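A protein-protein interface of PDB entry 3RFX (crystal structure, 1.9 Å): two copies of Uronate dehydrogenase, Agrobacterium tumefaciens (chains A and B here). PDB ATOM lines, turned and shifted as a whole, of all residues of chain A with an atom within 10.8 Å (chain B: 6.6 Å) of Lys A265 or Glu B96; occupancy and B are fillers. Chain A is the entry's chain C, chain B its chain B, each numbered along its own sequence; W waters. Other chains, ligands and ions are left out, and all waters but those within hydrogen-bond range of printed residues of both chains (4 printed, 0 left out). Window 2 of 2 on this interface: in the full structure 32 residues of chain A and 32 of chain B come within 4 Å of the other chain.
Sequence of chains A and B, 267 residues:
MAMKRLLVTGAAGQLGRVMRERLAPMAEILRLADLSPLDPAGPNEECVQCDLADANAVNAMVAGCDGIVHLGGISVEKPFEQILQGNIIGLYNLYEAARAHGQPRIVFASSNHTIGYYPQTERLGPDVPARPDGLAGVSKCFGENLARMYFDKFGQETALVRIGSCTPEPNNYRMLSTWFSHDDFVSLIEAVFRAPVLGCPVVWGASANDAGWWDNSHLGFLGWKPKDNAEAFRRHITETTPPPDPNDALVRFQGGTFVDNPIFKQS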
ATOM      1  N   GLU A  77      -5.670 -15.112  10.190  1.00  0.00           N
ATOM      2  CA  GLU A  77      -5.005 -14.032   9.475  1.00  0.00           C
ATOM      3  C   GLU A  77      -4.243 -14.591   8.276  1.00  0.00           C
ATOM      4  O   GLU A  77      -3.499 -15.564   8.400  1.00  0.00           O
ATOM      5  CB  GLU A  77      -4.088 -13.227  10.394  1.00  0.00           C
ATOM      6  CG  GLU A  77      -3.545 -11.964   9.758  1.00  0.00           C
ATOM      7  CD  GLU A  77      -4.582 -10.844   9.641  1.00  0.00           C
ATOM      8  OE1 GLU A  77      -5.767 -11.065   9.981  1.00  0.00           O
ATOM      9  OE2 GLU A  77      -4.202  -9.729   9.216  1.00  0.00           O
ATOM     10  N   LYS A  78      -4.454 -13.967   7.121  1.00  0.00           N
ATOM     11  CA  LYS A  78      -3.841 -14.371   5.859  1.00  0.00           C
ATOM     12  C   LYS A  78      -3.568 -13.108   5.061  1.00  0.00           C
ATOM     13  O   LYS A  78      -3.990 -12.017   5.460  1.00  0.00           O
ATOM     14  CB  LYS A  78      -4.783 -15.289   5.065  1.00  0.00           C
ATOM     15  CG  LYS A  78      -4.924 -16.695   5.642  1.00  0.00           C
ATOM     16  CD  LYS A  78      -4.503 -17.746   4.631  1.00  0.00           C
ATOM     17  CE  LYS A  78      -4.556 -19.156   5.209  1.00  0.00           C
ATOM     18  NZ  LYS A  78      -3.392 -19.433   6.092  1.00  0.00           N
ATOM     19  N   PRO A  79      -2.853 -13.236   3.936  1.00  0.00           N
ATOM     20  CA  PRO A  79      -2.627 -12.094   3.043  1.00  0.00           C
ATOM     21  C   PRO A  79      -3.931 -11.512   2.509  1.00  0.00           C
ATOM     22  O   PRO A  79      -4.936 -12.216   2.379  1.00  0.00           O
ATOM     23  CB  PRO A  79      -1.818 -12.704   1.896  1.00  0.00           C
ATOM     24  CG  PRO A  79      -1.138 -13.879   2.508  1.00  0.00           C
ATOM     25  CD  PRO A  79      -2.118 -14.436   3.490  1.00  0.00           C
ATOM     26  N   PHE A  80      -3.895 -10.225   2.191  1.00  0.00           N
ATOM     27  CA  PHE A  80      -5.081  -9.477   1.801  1.00  0.00           C
ATOM     28  C   PHE A  80      -5.766 -10.103   0.590  1.00  0.00           C
ATOM     29  O   PHE A  80      -6.997 -10.179   0.525  1.00  0.00           O
ATOM     30  CB  PHE A  80      -4.682  -8.023   1.518  1.00  0.00           C
ATOM     31  CG  PHE A  80      -5.827  -7.136   1.110  1.00  0.00           C
ATOM     32  CD1 PHE A  80      -6.834  -6.825   2.004  1.00  0.00           C
ATOM     33  CD2 PHE A  80      -5.879  -6.593  -0.166  1.00  0.00           C
ATOM     34  CE1 PHE A  80      -7.883  -5.995   1.625  1.00  0.00           C
ATOM     35  CE2 PHE A  80      -6.925  -5.768  -0.547  1.00  0.00           C
ATOM     36  CZ  PHE A  80      -7.921  -5.468   0.351  1.00  0.00           C
ATOM     37  N   GLU A  81      -4.967 -10.570  -0.364  1.00  0.00           N
ATOM     38  CA  GLU A  81      -5.515 -11.157  -1.585  1.00  0.00           C
ATOM     39  C   GLU A  81      -6.545 -12.259  -1.307  1.00  0.00           C
ATOM     40  O   GLU A  81      -7.630 -12.283  -1.896  1.00  0.00           O
ATOM     41  CB  GLU A  81      -4.381 -11.705  -2.463  1.00  0.00           C
ATOM     42  CG  GLU A  81      -3.507 -10.627  -3.130  1.00  0.00           C
ATOM     43  CD  GLU A  81      -2.533  -9.915  -2.179  1.00  0.00           C
ATOM     44  OE1 GLU A  81      -2.386 -10.334  -1.004  1.00  0.00           O
ATOM     45  OE2 GLU A  81      -1.900  -8.925  -2.624  1.00  0.00           O
ATOM     46  N   GLN A  82      -6.199 -13.180  -0.418  1.00  0.00           N
ATOM     47  CA  GLN A  82      -7.078 -14.296  -0.097  1.00  0.00           C
ATOM     48  C   GLN A  82      -8.341 -13.829   0.626  1.00  0.00           C
ATOM     49  O   GLN A  82      -9.439 -14.319   0.358  1.00  0.00           O
ATOM     50  CB  GLN A  82      -6.349 -15.312   0.777  1.00  0.00           C
ATOM     51  CG  GLN A  82      -5.031 -15.810   0.204  1.00  0.00           C
ATOM     52  CD  GLN A  82      -4.396 -16.867   1.090  1.00  0.00           C
ATOM     53  OE1 GLN A  82      -5.096 -17.641   1.748  1.00  0.00           O
ATOM     54  NE2 GLN A  82      -3.065 -16.903   1.115  1.00  0.00           N
ATOM     55  N   ILE A  83      -8.167 -12.893   1.553  1.00  0.00           N
ATOM     56  CA  ILE A  83      -9.274 -12.339   2.335  1.00  0.00           C
ATOM     57  C   ILE A  83     -10.245 -11.593   1.435  1.00  0.00           C
ATOM     58  O   ILE A  83     -11.468 -11.675   1.589  1.00  0.00           O
ATOM     59  CB  ILE A  83      -8.737 -11.347   3.384  1.00  0.00           C
ATOM     60  CG1 ILE A  83      -7.891 -12.072   4.429  1.00  0.00           C
ATOM     61  CG2 ILE A  83      -9.873 -10.580   4.036  1.00  0.00           C
ATOM     62  CD1 ILE A  83      -8.688 -12.883   5.376  1.00  0.00           C
ATOM     63  N   GLY A 134      -6.660  -7.464  12.915  1.00  0.00           N
ATOM     64  CA  GLY A 134      -5.929  -7.773  11.696  1.00  0.00           C
ATOM     65  C   GLY A 134      -6.844  -7.669  10.488  1.00  0.00           C
ATOM     66  O   GLY A 134      -7.991  -7.247  10.613  1.00  0.00           O
ATOM     67  N   LEU A 135      -6.346  -8.065   9.318  1.00  0.00           N
ATOM     68  CA  LEU A 135      -7.147  -7.992   8.101  1.00  0.00           C
ATOM     69  C   LEU A 135      -8.364  -8.911   8.143  1.00  0.00           C
ATOM     70  O   LEU A 135      -9.404  -8.592   7.561  1.00  0.00           O
ATOM     71  CB  LEU A 135      -6.291  -8.339   6.873  1.00  0.00           C
ATOM     72  CG  LEU A 135      -5.121  -7.388   6.599  1.00  0.00           C
ATOM     73  CD1 LEU A 135      -4.318  -7.888   5.404  1.00  0.00           C
ATOM     74  CD2 LEU A 135      -5.607  -5.963   6.368  1.00  0.00           C
ATOM     75  N   ASN A 261       0.015 -10.784  15.251  1.00  0.00           N
ATOM     76  CA  ASN A 261       0.225 -11.076  13.827  1.00  0.00           C
ATOM     77  C   ASN A 261       0.734  -9.857  13.081  1.00  0.00           C
ATOM     78  O   ASN A 261       0.259  -8.742  13.303  1.00  0.00           O
ATOM     79  CB  ASN A 261      -1.071 -11.527  13.137  1.00  0.00           C
ATOM     80  CG  ASN A 261      -1.502 -12.921  13.526  1.00  0.00           C
ATOM     81  OD1 ASN A 261      -0.678 -13.789  13.799  1.00  0.00           O
ATOM     82  ND2 ASN A 261      -2.814 -13.148  13.537  1.00  0.00           N
ATOM     83  N   PRO A 262       1.687 -10.065  12.163  1.00  0.00           N
ATOM     84  CA  PRO A 262       2.036  -8.987  11.238  1.00  0.00           C
ATOM     85  C   PRO A 262       1.011  -8.952  10.116  1.00  0.00           C
ATOM     86  O   PRO A 262       0.076  -9.761  10.119  1.00  0.00           O
ATOM     87  CB  PRO A 262       3.386  -9.444  10.677  1.00  0.00           C
ATOM     88  CG  PRO A 262       3.289 -10.933  10.683  1.00  0.00           C
ATOM     89  CD  PRO A 262       2.481 -11.285  11.923  1.00  0.00           C
ATOM     90  N   ILE A 263       1.171  -8.022   9.179  1.00  0.00           N
ATOM     91  CA  ILE A 263       0.428  -8.084   7.927  1.00  0.00           C
ATOM     92  C   ILE A 263       1.133  -9.109   7.042  1.00  0.00           C
ATOM     93  O   ILE A 263       2.257  -8.882   6.611  1.00  0.00           O
ATOM     94  CB  ILE A 263       0.406  -6.721   7.198  1.00  0.00           C
ATOM     95  CG1 ILE A 263      -0.221  -5.639   8.078  1.00  0.00           C
ATOM     96  CG2 ILE A 263      -0.367  -6.828   5.872  1.00  0.00           C
ATOM     97  CD1 ILE A 263      -1.678  -5.915   8.446  1.00  0.00           C
ATOM     98  N   PHE A 264       0.487 -10.239   6.786  1.00  0.00           N
ATOM     99  CA  PHE A 264       1.103 -11.294   5.983  1.00  0.00           C
ATOM    100  C   PHE A 264       1.080 -10.949   4.499  1.00  0.00           C
ATOM    101  O   PHE A 264       0.100 -10.406   3.992  1.00  0.00           O
ATOM    102  CB  PHE A 264       0.401 -12.636   6.210  1.00  0.00           C
ATOM    103  CG  PHE A 264       0.584 -13.200   7.593  1.00  0.00           C
ATOM    104  CD1 PHE A 264       1.828 -13.636   8.019  1.00  0.00           C
ATOM    105  CD2 PHE A 264      -0.497 -13.333   8.456  1.00  0.00           C
ATOM    106  CE1 PHE A 264       1.997 -14.170   9.292  1.00  0.00           C
ATOM    107  CE2 PHE A 264      -0.333 -13.875   9.723  1.00  0.00           C
ATOM    108  CZ  PHE A 264       0.918 -14.287  10.142  1.00  0.00           C
ATOM    109  N   LYS A 265       2.157 -11.277   3.798  1.00  0.00           N
ATOM    110  CA  LYS A 265       2.259 -10.952   2.376  1.00  0.00           C
ATOM    111  C   LYS A 265       2.282 -12.203   1.504  1.00  0.00           C
ATOM    112  O   LYS A 265       2.741 -13.264   1.934  1.00  0.00           O
ATOM    113  CB  LYS A 265       3.504 -10.108   2.108  1.00  0.00           C
ATOM    114  CG  LYS A 265       3.539  -8.783   2.854  1.00  0.00           C
ATOM    115  CD  LYS A 265       2.395  -7.873   2.435  1.00  0.00           C
ATOM    116  CE  LYS A 265       2.450  -6.530   3.160  1.00  0.00           C
ATOM    117  NZ  LYS A 265       2.919  -5.397   2.285  1.00  0.00           N
ATOM    118  N   GLN A 266       1.787 -12.061   0.278  1.00  0.00           N
ATOM    119  CA  GLN A 266       1.760 -13.156  -0.689  1.00  0.00           C
ATOM    120  C   GLN A 266       3.163 -13.436  -1.218  1.00  0.00           C
ATOM    121  O   GLN A 266       3.822 -14.389  -0.794  1.00  0.00           O
ATOM    122  CB  GLN A 266       0.829 -12.808  -1.854  1.00  0.00           C
ATOM    123  CG  GLN A 266       0.299 -14.008  -2.618  1.00  0.00           C
ATOM    124  CD  GLN A 266      -0.993 -14.554  -2.031  1.00  0.00           C
ATOM    125  OE1 GLN A 266      -1.837 -13.797  -1.545  1.00  0.00           O
ATOM    126  NE2 GLN A 266      -1.160 -15.875  -2.080  1.00  0.00           N
ATOM    127  N   ASN B  59       2.700   3.143  -3.461  1.00  0.00           N
ATOM    128  CA  ASN B  59       3.957   3.191  -2.720  1.00  0.00           C
ATOM    129  C   ASN B  59       4.776   4.418  -3.117  1.00  0.00           C
ATOM    130  O   ASN B  59       5.252   5.161  -2.254  1.00  0.00           O
ATOM    131  CB  ASN B  59       4.782   1.921  -2.952  1.00  0.00           C
ATOM    132  CG  ASN B  59       6.009   1.851  -2.062  1.00  0.00           C
ATOM    133  OD1 ASN B  59       7.121   2.184  -2.484  1.00  0.00           O
ATOM    134  ND2 ASN B  59       5.817   1.413  -0.820  1.00  0.00           N
ATOM    135  N   LEU B  91      -7.563   1.560  -0.183  1.00  0.00           N
ATOM    136  CA  LEU B  91      -7.279   1.891   1.217  1.00  0.00           C
ATOM    137  C   LEU B  91      -6.195   0.985   1.797  1.00  0.00           C
ATOM    138  O   LEU B  91      -5.278   1.444   2.481  1.00  0.00           O
ATOM    139  CB  LEU B  91      -8.565   1.775   2.048  1.00  0.00           C
ATOM    140  CG  LEU B  91      -9.200   3.112   2.430  1.00  0.00           C
ATOM    141  CD1 LEU B  91      -8.350   3.837   3.457  1.00  0.00           C
ATOM    142  CD2 LEU B  91      -9.388   3.979   1.189  1.00  0.00           C
ATOM    143  N   TYR B  92      -6.294  -0.309   1.521  1.00  0.00           N
ATOM    144  CA  TYR B  92      -5.229  -1.226   1.908  1.00  0.00           C
ATOM    145  C   TYR B  92      -3.890  -0.738   1.360  1.00  0.00           C
ATOM    146  O   TYR B  92      -2.905  -0.641   2.095  1.00  0.00           O
ATOM    147  CB  TYR B  92      -5.517  -2.651   1.417  1.00  0.00           C
ATOM    148  CG  TYR B  92      -4.364  -3.595   1.626  1.00  0.00           C
ATOM    149  CD1 TYR B  92      -4.030  -4.042   2.901  1.00  0.00           C
ATOM    150  CD2 TYR B  92      -3.591  -4.024   0.554  1.00  0.00           C
ATOM    151  CE1 TYR B  92      -2.964  -4.904   3.100  1.00  0.00           C
ATOM    152  CE2 TYR B  92      -2.527  -4.890   0.738  1.00  0.00           C
ATOM    153  CZ  TYR B  92      -2.220  -5.330   2.010  1.00  0.00           C
ATOM    154  OH  TYR B  92      -1.162  -6.194   2.190  1.00  0.00           O
ATOM    155  N   ASN B  93      -3.856  -0.432   0.065  1.00  0.00           N
ATOM    156  CA  ASN B  93      -2.621   0.035  -0.563  1.00  0.00           C
ATOM    157  C   ASN B  93      -2.087   1.311   0.095  1.00  0.00           C
ATOM    158  O   ASN B  93      -0.882   1.442   0.312  1.00  0.00           O
ATOM    159  CB  ASN B  93      -2.811   0.251  -2.070  1.00  0.00           C
ATOM    160  CG  ASN B  93      -2.938  -1.058  -2.831  1.00  0.00           C
ATOM    161  OD1 ASN B  93      -2.573  -2.110  -2.323  1.00  0.00           O
ATOM    162  ND2 ASN B  93      -3.462  -0.993  -4.054  1.00  0.00           N
ATOM    163  N   LEU B  94      -2.986   2.244   0.410  1.00  0.00           N
ATOM    164  CA  LEU B  94      -2.581   3.501   1.045  1.00  0.00           C
ATOM    165  C   LEU B  94      -1.960   3.247   2.408  1.00  0.00           C
ATOM    166  O   LEU B  94      -0.902   3.791   2.719  1.00  0.00           O
ATOM    167  CB  LEU B  94      -3.763   4.470   1.194  1.00  0.00           C
ATOM    168  CG  LEU B  94      -3.395   5.851   1.749  1.00  0.00           C
ATOM    169  CD1 LEU B  94      -2.616   6.667   0.712  1.00  0.00           C
ATOM    170  CD2 LEU B  94      -4.638   6.617   2.199  1.00  0.00           C
ATOM    171  N   TYR B  95      -2.615   2.418   3.222  1.00  0.00           N
ATOM    172  CA  TYR B  95      -2.105   2.146   4.566  1.00  0.00           C
ATOM    173  C   TYR B  95      -0.787   1.369   4.574  1.00  0.00           C
ATOM    174  O   TYR B  95       0.097   1.647   5.387  1.00  0.00           O
ATOM    175  CB  TYR B  95      -3.197   1.534   5.475  1.00  0.00           C
ATOM    176  CG  TYR B  95      -4.009   2.658   6.063  1.00  0.00           C
ATOM    177  CD1 TYR B  95      -3.761   3.129   7.356  1.00  0.00           C
ATOM    178  CD2 TYR B  95      -4.953   3.324   5.290  1.00  0.00           C
ATOM    179  CE1 TYR B  95      -4.468   4.218   7.871  1.00  0.00           C
ATOM    180  CE2 TYR B  95      -5.672   4.402   5.799  1.00  0.00           C
ATOM    181  CZ  TYR B  95      -5.420   4.843   7.090  1.00  0.00           C
ATOM    182  OH  TYR B  95      -6.119   5.928   7.585  1.00  0.00           O
ATOM    183  N   GLU B  96      -0.642   0.422   3.653  1.00  0.00           N
ATOM    184  CA  GLU B  96       0.620  -0.296   3.510  1.00  0.00           C
ATOM    185  C   GLU B  96       1.740   0.632   3.043  1.00  0.00           C
ATOM    186  O   GLU B  96       2.869   0.535   3.518  1.00  0.00           O
ATOM    187  CB  GLU B  96       0.465  -1.486   2.556  1.00  0.00           C
ATOM    188  CG  GLU B  96      -0.099  -2.729   3.248  1.00  0.00           C
ATOM    189  CD  GLU B  96       0.801  -3.193   4.375  1.00  0.00           C
ATOM    190  OE1 GLU B  96       1.889  -3.724   4.076  1.00  0.00           O
ATOM    191  OE2 GLU B  96       0.439  -3.009   5.563  1.00  0.00           O
ATOM    192  N   ALA B  97       1.420   1.531   2.120  1.00  0.00           N
ATOM    193  CA  ALA B  97       2.392   2.499   1.632  1.00  0.00           C
ATOM    194  C   ALA B  97       2.834   3.406   2.784  1.00  0.00           C
ATOM    195  O   ALA B  97       4.021   3.671   2.967  1.00  0.00           O
ATOM    196  CB  ALA B  97       1.799   3.313   0.509  1.00  0.00           C
ATOM    197  N   ALA B  98       1.871   3.871   3.571  1.00  0.00           N
ATOM    198  CA  ALA B  98       2.195   4.724   4.710  1.00  0.00           C
ATOM    199  C   ALA B  98       3.071   3.964   5.694  1.00  0.00           C
ATOM    200  O   ALA B  98       4.037   4.513   6.232  1.00  0.00           O
ATOM    201  CB  ALA B  98       0.914   5.234   5.390  1.00  0.00           C
ATOM    202  N   ARG B  99       2.749   2.692   5.914  1.00  0.00           N
ATOM    203  CA  ARG B  99       3.492   1.883   6.869  1.00  0.00           C
ATOM    204  C   ARG B  99       4.947   1.714   6.431  1.00  0.00           C
ATOM    205  O   ARG B  99       5.844   1.623   7.269  1.00  0.00           O
ATOM    206  CB  ARG B  99       2.818   0.521   7.078  1.00  0.00           C
ATOM    207  CG  ARG B  99       3.413  -0.314   8.207  1.00  0.00           C
ATOM    208  CD  ARG B  99       2.539  -1.524   8.546  1.00  0.00           C
ATOM    209  NE  ARG B  99       2.564  -2.559   7.513  1.00  0.00           N
ATOM    210  CZ  ARG B  99       3.494  -3.508   7.426  1.00  0.00           C
ATOM    211  NH1 ARG B  99       4.487  -3.547   8.308  1.00  0.00           N
ATOM    212  NH2 ARG B  99       3.439  -4.414   6.452  1.00  0.00           N
ATOM    213  N   ALA B 100       5.171   1.675   5.118  1.00  0.00           N
ATOM    214  CA  ALA B 100       6.515   1.475   4.575  1.00  0.00           C
ATOM    215  C   ALA B 100       7.316   2.771   4.516  1.00  0.00           C
ATOM    216  O   ALA B 100       8.520   2.750   4.246  1.00  0.00           O
ATOM    217  CB  ALA B 100       6.443   0.844   3.184  1.00  0.00           C
ATOM    218  N   HIS B 101       6.656   3.901   4.757  1.00  0.00           N
ATOM    219  CA  HIS B 101       7.303   5.194   4.576  1.00  0.00           C
ATOM    220  C   HIS B 101       7.081   6.154   5.741  1.00  0.00           C
ATOM    221  O   HIS B 101       6.748   7.314   5.536  1.00  0.00           O
ATOM    222  CB  HIS B 101       6.863   5.836   3.253  1.00  0.00           C
ATOM    223  CG  HIS B 101       7.299   5.062   2.045  1.00  0.00           C
ATOM    224  ND1 HIS B 101       8.593   5.097   1.570  1.00  0.00           N
ATOM    225  CD2 HIS B 101       6.623   4.213   1.234  1.00  0.00           C
ATOM    226  CE1 HIS B 101       8.693   4.309   0.512  1.00  0.00           C
ATOM    227  NE2 HIS B 101       7.512   3.760   0.287  1.00  0.00           N
ATOM    228  N   LEU B 146     -10.174  -0.370   8.889  1.00  0.00           N
ATOM    229  CA  LEU B 146      -8.774  -0.611   8.544  1.00  0.00           C
ATOM    230  C   LEU B 146      -7.860   0.381   9.265  1.00  0.00           C
ATOM    231  O   LEU B 146      -6.838  -0.005   9.828  1.00  0.00           O
ATOM    232  CB  LEU B 146      -8.557  -0.496   7.030  1.00  0.00           C
ATOM    233  CG  LEU B 146      -7.178  -0.957   6.522  1.00  0.00           C
ATOM    234  CD1 LEU B 146      -7.103  -2.476   6.485  1.00  0.00           C
ATOM    235  CD2 LEU B 146      -6.876  -0.391   5.149  1.00  0.00           C
ATOM    236  N   TYR B 150      -4.736  -0.391  11.895  1.00  0.00           N
ATOM    237  CA  TYR B 150      -3.352   0.094  11.744  1.00  0.00           C
ATOM    238  C   TYR B 150      -2.950   0.967  12.925  1.00  0.00           C
ATOM    239  O   TYR B 150      -1.786   0.977  13.347  1.00  0.00           O
ATOM    240  CB  TYR B 150      -3.149   0.848  10.418  1.00  0.00           C
ATOM    241  CG  TYR B 150      -2.867  -0.099   9.253  1.00  0.00           C
ATOM    242  CD1 TYR B 150      -1.579  -0.251   8.746  1.00  0.00           C
ATOM    243  CD2 TYR B 150      -3.883  -0.878   8.707  1.00  0.00           C
ATOM    244  CE1 TYR B 150      -1.318  -1.135   7.698  1.00  0.00           C
ATOM    245  CE2 TYR B 150      -3.636  -1.762   7.667  1.00  0.00           C
ATOM    246  CZ  TYR B 150      -2.351  -1.886   7.166  1.00  0.00           C
ATOM    247  OH  TYR B 150      -2.108  -2.756   6.122  1.00  0.00           O
ATOM    248  N   PHE B 154       0.080  -0.698  14.716  1.00  0.00           N
ATOM    249  CA  PHE B 154       1.334  -0.041  14.336  1.00  0.00           C
ATOM    250  C   PHE B 154       1.492   1.401  14.817  1.00  0.00           C
ATOM    251  O   PHE B 154       2.577   1.980  14.698  1.00  0.00           O
ATOM    252  CB  PHE B 154       1.508  -0.072  12.819  1.00  0.00           C
ATOM    253  CG  PHE B 154       1.493  -1.458  12.235  1.00  0.00           C
ATOM    254  CD1 PHE B 154       2.558  -2.316  12.427  1.00  0.00           C
ATOM    255  CD2 PHE B 154       0.406  -1.900  11.494  1.00  0.00           C
ATOM    256  CE1 PHE B 154       2.549  -3.592  11.891  1.00  0.00           C
ATOM    257  CE2 PHE B 154       0.392  -3.180  10.952  1.00  0.00           C
ATOM    258  CZ  PHE B 154       1.466  -4.023  11.151  1.00  0.00           C
HETATM  259  O   HOH W   1       0.640  -6.489   0.065  1.00  0.00           O
HETATM  260  O   HOH W   2      -1.413  -8.778   2.623  1.00  0.00           O
HETATM  261  O   HOH W   3       4.461  -7.333   6.761  1.00  0.00           O
HETATM  262  O   HOH W   4       3.532  -6.508   9.435  1.00  0.00           O
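No position is printed for both chains. Of the 9 pairs that touch across the chains among the printed residues, none has its exchanged pair printed and touching as well.
Hydrophobic or aromatic side chains of chain A within 4 Å of the printed part of chain B: Phe A80, Leu A135 and Ile A263. Printed residues of chain B that touch a printed residue of chain A: Tyr B92, Glu B96, Arg B99, Leu B146, Tyr B150 and Phe B154. Among the printed residues, Asp or Glu carboxylates within 4 Å of a Lys or Arg side-chain nitrogen of the other chain: Lys A265 with Glu B96.
OE1 of Glu B96 lies within salt-bridge range of NZ of Lys A265 (2.7 Å).
Phe A80 touches Tyr B92. Leu A135 touches Leu B146. Tyr B92 touches Ile A263. OE2 of Glu B96 touches CG1 of Ile A263 (3.7 Å). Arg B99 touches Ile A263. CD1 of Ile A263 touches OH of Tyr B150, at 3.9 Å. CG1 of Ile A263 touches CE2 of Phe B154, 3.8 Å away. Tyr B92 touches Lys A265.
Of the printed residues of chain B, Lys A265 touches Tyr B92 (3.8 Å) and Glu B96 (2.7 Å). Of chain A, only Ile A263 and Lys A265 come within 4 Å of Glu B96. Ala B97 touches none of the printed residues of chain A. No residue of chain A comes within 4 Å of Ala B100. Of the printed residues of chain A, Tyr B150 touches Ile A263 (3.9 Å). Of the printed residues of chain B, Ile A263 touches Tyr B92 (3.8 Å), Glu B96 (3.7 Å), Arg B99 (3.9 Å), Tyr B150 (3.9 Å) and Phe B154 (3.8 Å). Of the printed residues of chain B, Leu A135 touches Leu B146 (3.8 Å). Of the printed residues of chain B, Phe A80 touches Tyr B92 (3.5 Å). The nearest residue of chain B that does not touch Lys A265 is Arg B99 (4.04 Å).
OE2 of Glu B96 lies within salt-bridge range of NE of Arg B99 (2.9 Å). The side-chain carboxylate of Glu B96 lies within hydrogen-bond range of the side-chain hydroxyl of Tyr B150. OE2 of Glu A77 lies within hydrogen-bond range of N of Leu A135, 2.7 Å away.
Water W2 lies within hydrogen-bond range of O of Phe A264, OH of Tyr B92 and N of Phe A80. Water W3 lies within hydrogen-bond range of O of Ile A263 and NH2 of Arg B99. Water W1 bridges the side-chain hydroxyl (OH) of Tyr B92 (2.8 Å) and the side-chain amino group (NZ) of Lys A265 (3.4 Å). Water W4 bridges N of Ile A263 (2.8 Å) and NH1 of Arg B99 (3.3 Å).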
